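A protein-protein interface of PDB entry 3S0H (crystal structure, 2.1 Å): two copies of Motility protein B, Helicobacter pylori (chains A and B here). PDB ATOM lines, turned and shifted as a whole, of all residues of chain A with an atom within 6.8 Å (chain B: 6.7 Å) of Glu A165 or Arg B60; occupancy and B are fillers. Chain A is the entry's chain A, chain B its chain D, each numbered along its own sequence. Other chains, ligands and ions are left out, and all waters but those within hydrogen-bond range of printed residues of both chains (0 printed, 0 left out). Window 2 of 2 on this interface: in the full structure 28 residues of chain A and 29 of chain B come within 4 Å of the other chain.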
ATOM      1  N   SER A 160      14.876   5.408  22.326  1.00  0.00           N
ATOM      2  CA  SER A 160      15.284   6.384  21.324  1.00  0.00           C
ATOM      3  C   SER A 160      15.452   5.715  19.974  1.00  0.00           C
ATOM      4  O   SER A 160      14.954   6.209  18.975  1.00  0.00           O
ATOM      5  CB  SER A 160      16.569   7.105  21.767  1.00  0.00           C
ATOM      6  OG  SER A 160      16.998   8.025  20.775  1.00  0.00           O
ATOM      7  N   ILE A 161      16.129   4.568  19.951  1.00  0.00           N
ATOM      8  CA  ILE A 161      16.314   3.821  18.696  1.00  0.00           C
ATOM      9  C   ILE A 161      14.964   3.486  18.010  1.00  0.00           C
ATOM     10  O   ILE A 161      14.742   3.771  16.791  1.00  0.00           O
ATOM     11  CB  ILE A 161      17.210   2.534  18.917  1.00  0.00           C
ATOM     12  CG1 ILE A 161      18.638   2.960  19.271  1.00  0.00           C
ATOM     13  CG2 ILE A 161      17.250   1.648  17.665  1.00  0.00           C
ATOM     14  CD1 ILE A 161      19.491   1.892  19.872  1.00  0.00           C
ATOM     15  N   LEU A 162      14.068   2.895  18.798  1.00  0.00           N
ATOM     16  CA  LEU A 162      12.751   2.480  18.303  1.00  0.00           C
ATOM     17  C   LEU A 162      11.929   3.685  17.825  1.00  0.00           C
ATOM     18  O   LEU A 162      11.235   3.623  16.797  1.00  0.00           O
ATOM     19  CB  LEU A 162      12.005   1.694  19.385  1.00  0.00           C
ATOM     20  CG  LEU A 162      12.547   0.276  19.597  1.00  0.00           C
ATOM     21  CD1 LEU A 162      11.967  -0.380  20.814  1.00  0.00           C
ATOM     22  CD2 LEU A 162      12.268  -0.546  18.378  1.00  0.00           C
ATOM     23  N   ASP A 163      12.036   4.768  18.587  1.00  0.00           N
ATOM     24  CA  ASP A 163      11.386   6.024  18.298  1.00  0.00           C
ATOM     25  C   ASP A 163      11.850   6.638  16.988  1.00  0.00           C
ATOM     26  O   ASP A 163      11.021   7.109  16.197  1.00  0.00           O
ATOM     27  CB  ASP A 163      11.644   7.019  19.428  1.00  0.00           C
ATOM     28  CG  ASP A 163      10.917   8.311  19.216  1.00  0.00           C
ATOM     29  OD1 ASP A 163      11.592   9.309  18.854  1.00  0.00           O
ATOM     30  OD2 ASP A 163       9.665   8.314  19.344  1.00  0.00           O
ATOM     31  N   ASN A 164      13.159   6.657  16.753  1.00  0.00           N
ATOM     32  CA  ASN A 164      13.661   7.224  15.507  1.00  0.00           C
ATOM     33  C   ASN A 164      13.233   6.444  14.265  1.00  0.00           C
ATOM     34  O   ASN A 164      12.987   7.037  13.215  1.00  0.00           O
ATOM     35  CB  ASN A 164      15.174   7.433  15.560  1.00  0.00           C
ATOM     36  CG  ASN A 164      15.565   8.635  16.409  1.00  0.00           C
ATOM     37  OD1 ASN A 164      16.705   8.744  16.898  1.00  0.00           O
ATOM     38  ND2 ASN A 164      14.618   9.541  16.600  1.00  0.00           N
ATOM     39  N   GLU A 165      13.098   5.127  14.399  1.00  0.00           N
ATOM     40  CA  GLU A 165      12.712   4.285  13.274  1.00  0.00           C
ATOM     41  C   GLU A 165      11.204   4.250  13.023  1.00  0.00           C
ATOM     42  O   GLU A 165      10.772   4.261  11.873  1.00  0.00           O
ATOM     43  CB  GLU A 165      13.253   2.871  13.463  1.00  0.00           C
ATOM     44  CG  GLU A 165      12.763   1.861  12.435  1.00  0.00           C
ATOM     45  CD  GLU A 165      13.236   2.145  11.010  1.00  0.00           C
ATOM     46  OE1 GLU A 165      14.385   2.578  10.801  1.00  0.00           O
ATOM     47  OE2 GLU A 165      12.445   1.893  10.080  1.00  0.00           O
ATOM     48  N   PHE A 166      10.422   4.229  14.100  1.00  0.00           N
ATOM     49  CA  PHE A 166       8.987   3.937  14.034  1.00  0.00           C
ATOM     50  C   PHE A 166       8.010   5.104  14.306  1.00  0.00           C
ATOM     51  O   PHE A 166       6.828   4.972  14.044  1.00  0.00           O
ATOM     52  CB  PHE A 166       8.641   2.706  14.890  1.00  0.00           C
ATOM     53  CG  PHE A 166       9.224   1.424  14.361  1.00  0.00           C
ATOM     54  CD1 PHE A 166       8.747   0.853  13.182  1.00  0.00           C
ATOM     55  CD2 PHE A 166      10.255   0.785  15.039  1.00  0.00           C
ATOM     56  CE1 PHE A 166       9.305  -0.330  12.679  1.00  0.00           C
ATOM     57  CE2 PHE A 166      10.809  -0.402  14.553  1.00  0.00           C
ATOM     58  CZ  PHE A 166      10.338  -0.961  13.380  1.00  0.00           C
ATOM     59  N   ASN A 167       8.479   6.239  14.814  1.00  0.00           N
ATOM     60  CA  ASN A 167       7.609   7.428  14.869  1.00  0.00           C
ATOM     61  C   ASN A 167       7.376   8.096  13.504  1.00  0.00           C
ATOM     62  O   ASN A 167       8.336   8.435  12.815  1.00  0.00           O
ATOM     63  CB  ASN A 167       8.106   8.451  15.899  1.00  0.00           C
ATOM     64  CG  ASN A 167       7.240   8.488  17.140  1.00  0.00           C
ATOM     65  OD1 ASN A 167       7.199   9.503  17.848  1.00  0.00           O
ATOM     66  ND2 ASN A 167       6.520   7.385  17.403  1.00  0.00           N
ATOM     67  N   PRO A 168       6.094   8.274  13.116  1.00  0.00           N
ATOM     68  CA  PRO A 168       5.650   8.948  11.884  1.00  0.00           C
ATOM     69  C   PRO A 168       5.443  10.445  12.095  1.00  0.00           C
ATOM     70  O   PRO A 168       5.297  11.198  11.122  1.00  0.00           O
ATOM     71  CB  PRO A 168       4.308   8.277  11.586  1.00  0.00           C
ATOM     72  CG  PRO A 168       3.749   7.951  12.936  1.00  0.00           C
ATOM     73  CD  PRO A 168       4.942   7.791  13.897  1.00  0.00           C
ATOM     74  N   THR B  15       4.617   3.886  11.592  1.00  0.00           N
ATOM     75  CA  THR B  15       4.583   3.497  10.163  1.00  0.00           C
ATOM     76  C   THR B  15       5.976   2.980   9.744  1.00  0.00           C
ATOM     77  O   THR B  15       6.905   2.993  10.556  1.00  0.00           O
ATOM     78  CB  THR B  15       4.139   4.697   9.239  1.00  0.00           C
ATOM     79  OG1 THR B  15       2.809   5.119   9.579  1.00  0.00           O
ATOM     80  CG2 THR B  15       4.156   4.316   7.763  1.00  0.00           C
ATOM     81  N   ILE B  16       6.104   2.506   8.498  1.00  0.00           N
ATOM     82  CA  ILE B  16       7.411   2.190   7.881  1.00  0.00           C
ATOM     83  C   ILE B  16       7.404   2.174   6.340  1.00  0.00           C
ATOM     84  O   ILE B  16       6.452   1.689   5.713  1.00  0.00           O
ATOM     85  CB  ILE B  16       8.049   0.889   8.446  1.00  0.00           C
ATOM     86  CG1 ILE B  16       9.117   1.225   9.490  1.00  0.00           C
ATOM     87  CG2 ILE B  16       8.632   0.023   7.338  1.00  0.00           C
ATOM     88  CD1 ILE B  16       9.823   2.548   9.267  1.00  0.00           C
ATOM     89  N   ALA B  17       8.484   2.708   5.756  1.00  0.00           N
ATOM     90  CA  ALA B  17       8.617   2.918   4.311  1.00  0.00           C
ATOM     91  C   ALA B  17       7.421   3.687   3.755  1.00  0.00           C
ATOM     92  O   ALA B  17       7.197   3.726   2.538  1.00  0.00           O
ATOM     93  CB  ALA B  17       8.814   1.589   3.575  1.00  0.00           C
ATOM     94  N   ARG B  18       6.677   4.310   4.673  1.00  0.00           N
ATOM     95  CA  ARG B  18       5.395   4.975   4.400  1.00  0.00           C
ATOM     96  C   ARG B  18       4.283   3.994   3.986  1.00  0.00           C
ATOM     97  O   ARG B  18       3.514   4.262   3.056  1.00  0.00           O
ATOM     98  CB  ARG B  18       5.551   6.142   3.406  1.00  0.00           C
ATOM     99  CG  ARG B  18       6.285   7.365   3.968  1.00  0.00           C
ATOM    100  CD  ARG B  18       7.800   7.292   3.744  1.00  0.00           C
ATOM    101  NE  ARG B  18       8.515   8.358   4.449  1.00  0.00           N
ATOM    102  CZ  ARG B  18       9.076   8.227   5.651  1.00  0.00           C
ATOM    103  NH1 ARG B  18       9.016   7.073   6.298  1.00  0.00           N
ATOM    104  NH2 ARG B  18       9.705   9.256   6.206  1.00  0.00           N
ATOM    105  N   MET B  55       5.550  -8.474   5.449  1.00  0.00           N
ATOM    106  CA  MET B  55       6.855  -9.057   5.729  1.00  0.00           C
ATOM    107  C   MET B  55       7.924  -7.964   5.736  1.00  0.00           C
ATOM    108  O   MET B  55       8.987  -8.121   6.341  1.00  0.00           O
ATOM    109  CB  MET B  55       7.200 -10.116   4.675  1.00  0.00           C
ATOM    110  CG  MET B  55       6.278 -11.351   4.650  1.00  0.00           C
ATOM    111  SD  MET B  55       6.422 -12.418   6.107  1.00  0.00           S
ATOM    112  CE  MET B  55       7.910 -13.325   5.715  1.00  0.00           C
ATOM    113  N   LEU B  56       7.630  -6.854   5.071  1.00  0.00           N
ATOM    114  CA  LEU B  56       8.578  -5.748   4.984  1.00  0.00           C
ATOM    115  C   LEU B  56       8.642  -4.933   6.281  1.00  0.00           C
ATOM    116  O   LEU B  56       9.706  -4.410   6.638  1.00  0.00           O
ATOM    117  CB  LEU B  56       8.302  -4.876   3.738  1.00  0.00           C
ATOM    118  CG  LEU B  56       9.056  -3.557   3.492  1.00  0.00           C
ATOM    119  CD1 LEU B  56      10.556  -3.606   3.863  1.00  0.00           C
ATOM    120  CD2 LEU B  56       8.891  -3.147   2.040  1.00  0.00           C
ATOM    121  N   TYR B  57       7.520  -4.847   6.996  1.00  0.00           N
ATOM    122  CA  TYR B  57       7.506  -4.208   8.318  1.00  0.00           C
ATOM    123  C   TYR B  57       8.243  -5.078   9.340  1.00  0.00           C
ATOM    124  O   TYR B  57       8.954  -4.561  10.201  1.00  0.00           O
ATOM    125  CB  TYR B  57       6.067  -3.927   8.774  1.00  0.00           C
ATOM    126  CG  TYR B  57       5.948  -2.949   9.925  1.00  0.00           C
ATOM    127  CD1 TYR B  57       6.080  -1.570   9.709  1.00  0.00           C
ATOM    128  CD2 TYR B  57       5.698  -3.395  11.221  1.00  0.00           C
ATOM    129  CE1 TYR B  57       5.980  -0.665  10.757  1.00  0.00           C
ATOM    130  CE2 TYR B  57       5.593  -2.507  12.275  1.00  0.00           C
ATOM    131  CZ  TYR B  57       5.735  -1.139  12.035  1.00  0.00           C
ATOM    132  OH  TYR B  57       5.624  -0.234  13.069  1.00  0.00           O
ATOM    133  N   ILE B  58       8.079  -6.394   9.223  1.00  0.00           N
ATOM    134  CA  ILE B  58       8.764  -7.351  10.098  1.00  0.00           C
ATOM    135  C   ILE B  58      10.261  -7.206   9.881  1.00  0.00           C
ATOM    136  O   ILE B  58      10.999  -6.996  10.830  1.00  0.00           O
ATOM    137  CB  ILE B  58       8.331  -8.831   9.884  1.00  0.00           C
ATOM    138  CG1 ILE B  58       6.815  -8.952   9.700  1.00  0.00           C
ATOM    139  CG2 ILE B  58       8.798  -9.710  11.072  1.00  0.00           C
ATOM    140  CD1 ILE B  58       6.035  -9.159  11.011  1.00  0.00           C
ATOM    141  N   GLU B  59      10.679  -7.241   8.618  1.00  0.00           N
ATOM    142  CA  GLU B  59      12.079  -7.049   8.237  1.00  0.00           C
ATOM    143  C   GLU B  59      12.723  -5.821   8.892  1.00  0.00           C
ATOM    144  O   GLU B  59      13.826  -5.910   9.438  1.00  0.00           O
ATOM    145  CB  GLU B  59      12.196  -6.952   6.716  1.00  0.00           C
ATOM    146  CG  GLU B  59      13.609  -7.078   6.186  1.00  0.00           C
ATOM    147  CD  GLU B  59      13.671  -6.947   4.669  1.00  0.00           C
ATOM    148  OE1 GLU B  59      13.025  -6.027   4.118  1.00  0.00           O
ATOM    149  OE2 GLU B  59      14.370  -7.762   4.027  1.00  0.00           O
ATOM    150  N   ARG B  60      12.022  -4.692   8.855  1.00  0.00           N
ATOM    151  CA  ARG B  60      12.495  -3.457   9.492  1.00  0.00           C
ATOM    152  C   ARG B  60      12.768  -3.650  10.954  1.00  0.00           C
ATOM    153  O   ARG B  60      13.849  -3.348  11.410  1.00  0.00           O
ATOM    154  CB  ARG B  60      11.495  -2.315   9.328  1.00  0.00           C
ATOM    155  CG  ARG B  60      11.132  -1.993   7.858  1.00  0.00           C
ATOM    156  CD  ARG B  60      12.331  -1.647   6.967  1.00  0.00           C
ATOM    157  NE  ARG B  60      13.378  -0.895   7.673  1.00  0.00           N
ATOM    158  CZ  ARG B  60      13.494   0.433   7.707  1.00  0.00           C
ATOM    159  NH1 ARG B  60      14.501   0.985   8.382  1.00  0.00           N
ATOM    160  NH2 ARG B  60      12.625   1.218   7.072  1.00  0.00           N
ATOM    161  N   ILE B  61      11.774  -4.146  11.681  1.00  0.00           N
ATOM    162  CA  ILE B  61      11.936  -4.526  13.078  1.00  0.00           C
ATOM    163  C   ILE B  61      13.179  -5.441  13.218  1.00  0.00           C
ATOM    164  O   ILE B  61      14.017  -5.225  14.075  1.00  0.00           O
ATOM    165  CB  ILE B  61      10.657  -5.249  13.613  1.00  0.00           C
ATOM    166  CG1 ILE B  61       9.430  -4.327  13.519  1.00  0.00           C
ATOM    167  CG2 ILE B  61      10.862  -5.808  15.068  1.00  0.00           C
ATOM    168  CD1 ILE B  61       8.113  -5.043  13.744  1.00  0.00           C
ATOM    169  N   ALA B  62      13.296  -6.448  12.367  1.00  0.00           N
ATOM    170  CA  ALA B  62      14.419  -7.363  12.453  1.00  0.00           C
ATOM    171  C   ALA B  62      15.726  -6.587  12.290  1.00  0.00           C
ATOM    172  O   ALA B  62      16.697  -6.828  13.014  1.00  0.00           O
ATOM    173  CB  ALA B  62      14.300  -8.436  11.430  1.00  0.00           C
ATOM    174  N   LYS B  63      15.719  -5.610  11.375  1.00  0.00           N
ATOM    175  CA  LYS B  63      16.911  -4.826  11.111  1.00  0.00           C
ATOM    176  C   LYS B  63      17.339  -4.071  12.364  1.00  0.00           C
ATOM    177  O   LYS B  63      18.516  -4.074  12.732  1.00  0.00           O
ATOM    178  CB  LYS B  63      16.692  -3.878   9.917  1.00  0.00           C
ATOM    179  CG  LYS B  63      17.983  -3.440   9.191  1.00  0.00           C
ATOM    180  CD  LYS B  63      17.790  -2.167   8.307  1.00  0.00           C
ATOM    181  CE  LYS B  63      17.466  -0.889   9.131  1.00  0.00           C
ATOM    182  NZ  LYS B  63      18.569  -0.412  10.042  1.00  0.00           N
ATOM    183  N   ILE B  64      16.389  -3.424  13.025  1.00  0.00           N
ATOM    184  CA  ILE B  64      16.694  -2.758  14.292  1.00  0.00           C
ATOM    185  C   ILE B  64      17.187  -3.696  15.405  1.00  0.00           C
ATOM    186  O   ILE B  64      18.163  -3.363  16.098  1.00  0.00           O
ATOM    187  CB  ILE B  64      15.508  -1.923  14.779  1.00  0.00           C
ATOM    188  CG1 ILE B  64      15.445  -0.659  13.932  1.00  0.00           C
ATOM    189  CG2 ILE B  64      15.678  -1.578  16.284  1.00  0.00           C
ATOM    190  CD1 ILE B  64      14.086  -0.333  13.512  1.00  0.00           C
ATOM    191  N   ILE B  65      16.547  -4.860  15.569  1.00  0.00           N
ATOM    192  CA  ILE B  65      16.932  -5.795  16.644  1.00  0.00           C
ATOM    193  C   ILE B  65      18.394  -6.172  16.496  1.00  0.00           C
ATOM    194  O   ILE B  65      19.111  -6.246  17.482  1.00  0.00           O
ATOM    195  CB  ILE B  65      16.094  -7.095  16.666  1.00  0.00           C
ATOM    196  CG1 ILE B  65      14.732  -6.855  17.314  1.00  0.00           C
ATOM    197  CG2 ILE B  65      16.848  -8.223  17.415  1.00  0.00           C
ATOM    198  CD1 ILE B  65      13.625  -7.806  16.823  1.00  0.00           C
ATOM    199  N   LEU B 108      10.934 -13.025  12.336  1.00  0.00           N
ATOM    200  CA  LEU B 108      12.091 -12.259  12.796  1.00  0.00           C
ATOM    201  C   LEU B 108      13.353 -13.116  12.614  1.00  0.00           C
ATOM    202  O   LEU B 108      14.345 -12.663  12.032  1.00  0.00           O
ATOM    203  CB  LEU B 108      11.897 -11.795  14.238  1.00  0.00           C
ATOM    204  CG  LEU B 108      10.839 -10.709  14.468  1.00  0.00           C
ATOM    205  CD1 LEU B 108      10.556 -10.509  15.941  1.00  0.00           C
ATOM    206  CD2 LEU B 108      11.290  -9.379  13.829  1.00  0.00           C
ATOM    207  N   TYR B 111      14.517 -13.383   9.146  1.00  0.00           N
ATOM    208  CA  TYR B 111      15.197 -12.182   8.673  1.00  0.00           C
ATOM    209  C   TYR B 111      16.541 -11.919   9.343  1.00  0.00           C
ATOM    210  O   TYR B 111      17.046 -10.797   9.294  1.00  0.00           O
ATOM    211  CB  TYR B 111      14.283 -10.954   8.766  1.00  0.00           C
ATOM    212  CG  TYR B 111      13.265 -10.824   7.635  1.00  0.00           C
ATOM    213  CD1 TYR B 111      13.672 -10.656   6.300  1.00  0.00           C
ATOM    214  CD2 TYR B 111      11.905 -10.834   7.905  1.00  0.00           C
ATOM    215  CE1 TYR B 111      12.718 -10.528   5.264  1.00  0.00           C
ATOM    216  CE2 TYR B 111      10.954 -10.713   6.900  1.00  0.00           C
ATOM    217  CZ  TYR B 111      11.354 -10.554   5.586  1.00  0.00           C
ATOM    218  OH  TYR B 111      10.392 -10.430   4.621  1.00  0.00           O
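The side-chain carboxylate (OE2) of Glu A165 is in salt-bridge range of the guanidinium group (NH1) of Arg B60.
N of Thr B15 is in hydrogen-bond range of O of Phe A166 (3.5 Å).
Among the printed residues, merely in contact across the chains: Glu A165 with Ile B64 (2.8 Å), Glu A165 with Ile B16 (2.8 Å), Phe A166 with Tyr B57 (3.3 Å), Phe A166 with Ile B64 (3.4 Å), Phe A166 with Ile B61 (3.5 Å), Phe A166 with Ile B16 (3.6 Å) and Ile A161 with Ile B64 (3.8 Å).
Glu A165 touches just these residues of chain B: Ile B16, Arg B60 and Ile B64.
Of chain A, only Glu A165 (2.8 Å) comes within 4 Å of Arg B60.
Printed residues of chain B within 4 Å of Phe A166: Thr B15, Ile B16, Tyr B57, Ile B61 and Ile B64.
Printed residues of chain A within 4 Å of Ile B16: Glu A165 (2.8 Å) and Phe A166 (3.6 Å).
Ile B65 touches none of the printed residues of chain A.
The nearest residue of chain B that does not touch Glu A165 is Thr B15 (4.3 Å).
Printed residues of chain A that touch a printed residue of chain B: Ile A161, Glu A165 and Phe A166.
Of the 17 printed residues of chain B, 6 touch a printed residue of chain A.
Among the printed residues, 9 pairs touch across the chains.
No position is printed for both chains.
Of the 9 pairs that touch across the chains among the printed residues, none has its exchanged pair printed and touching as well.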
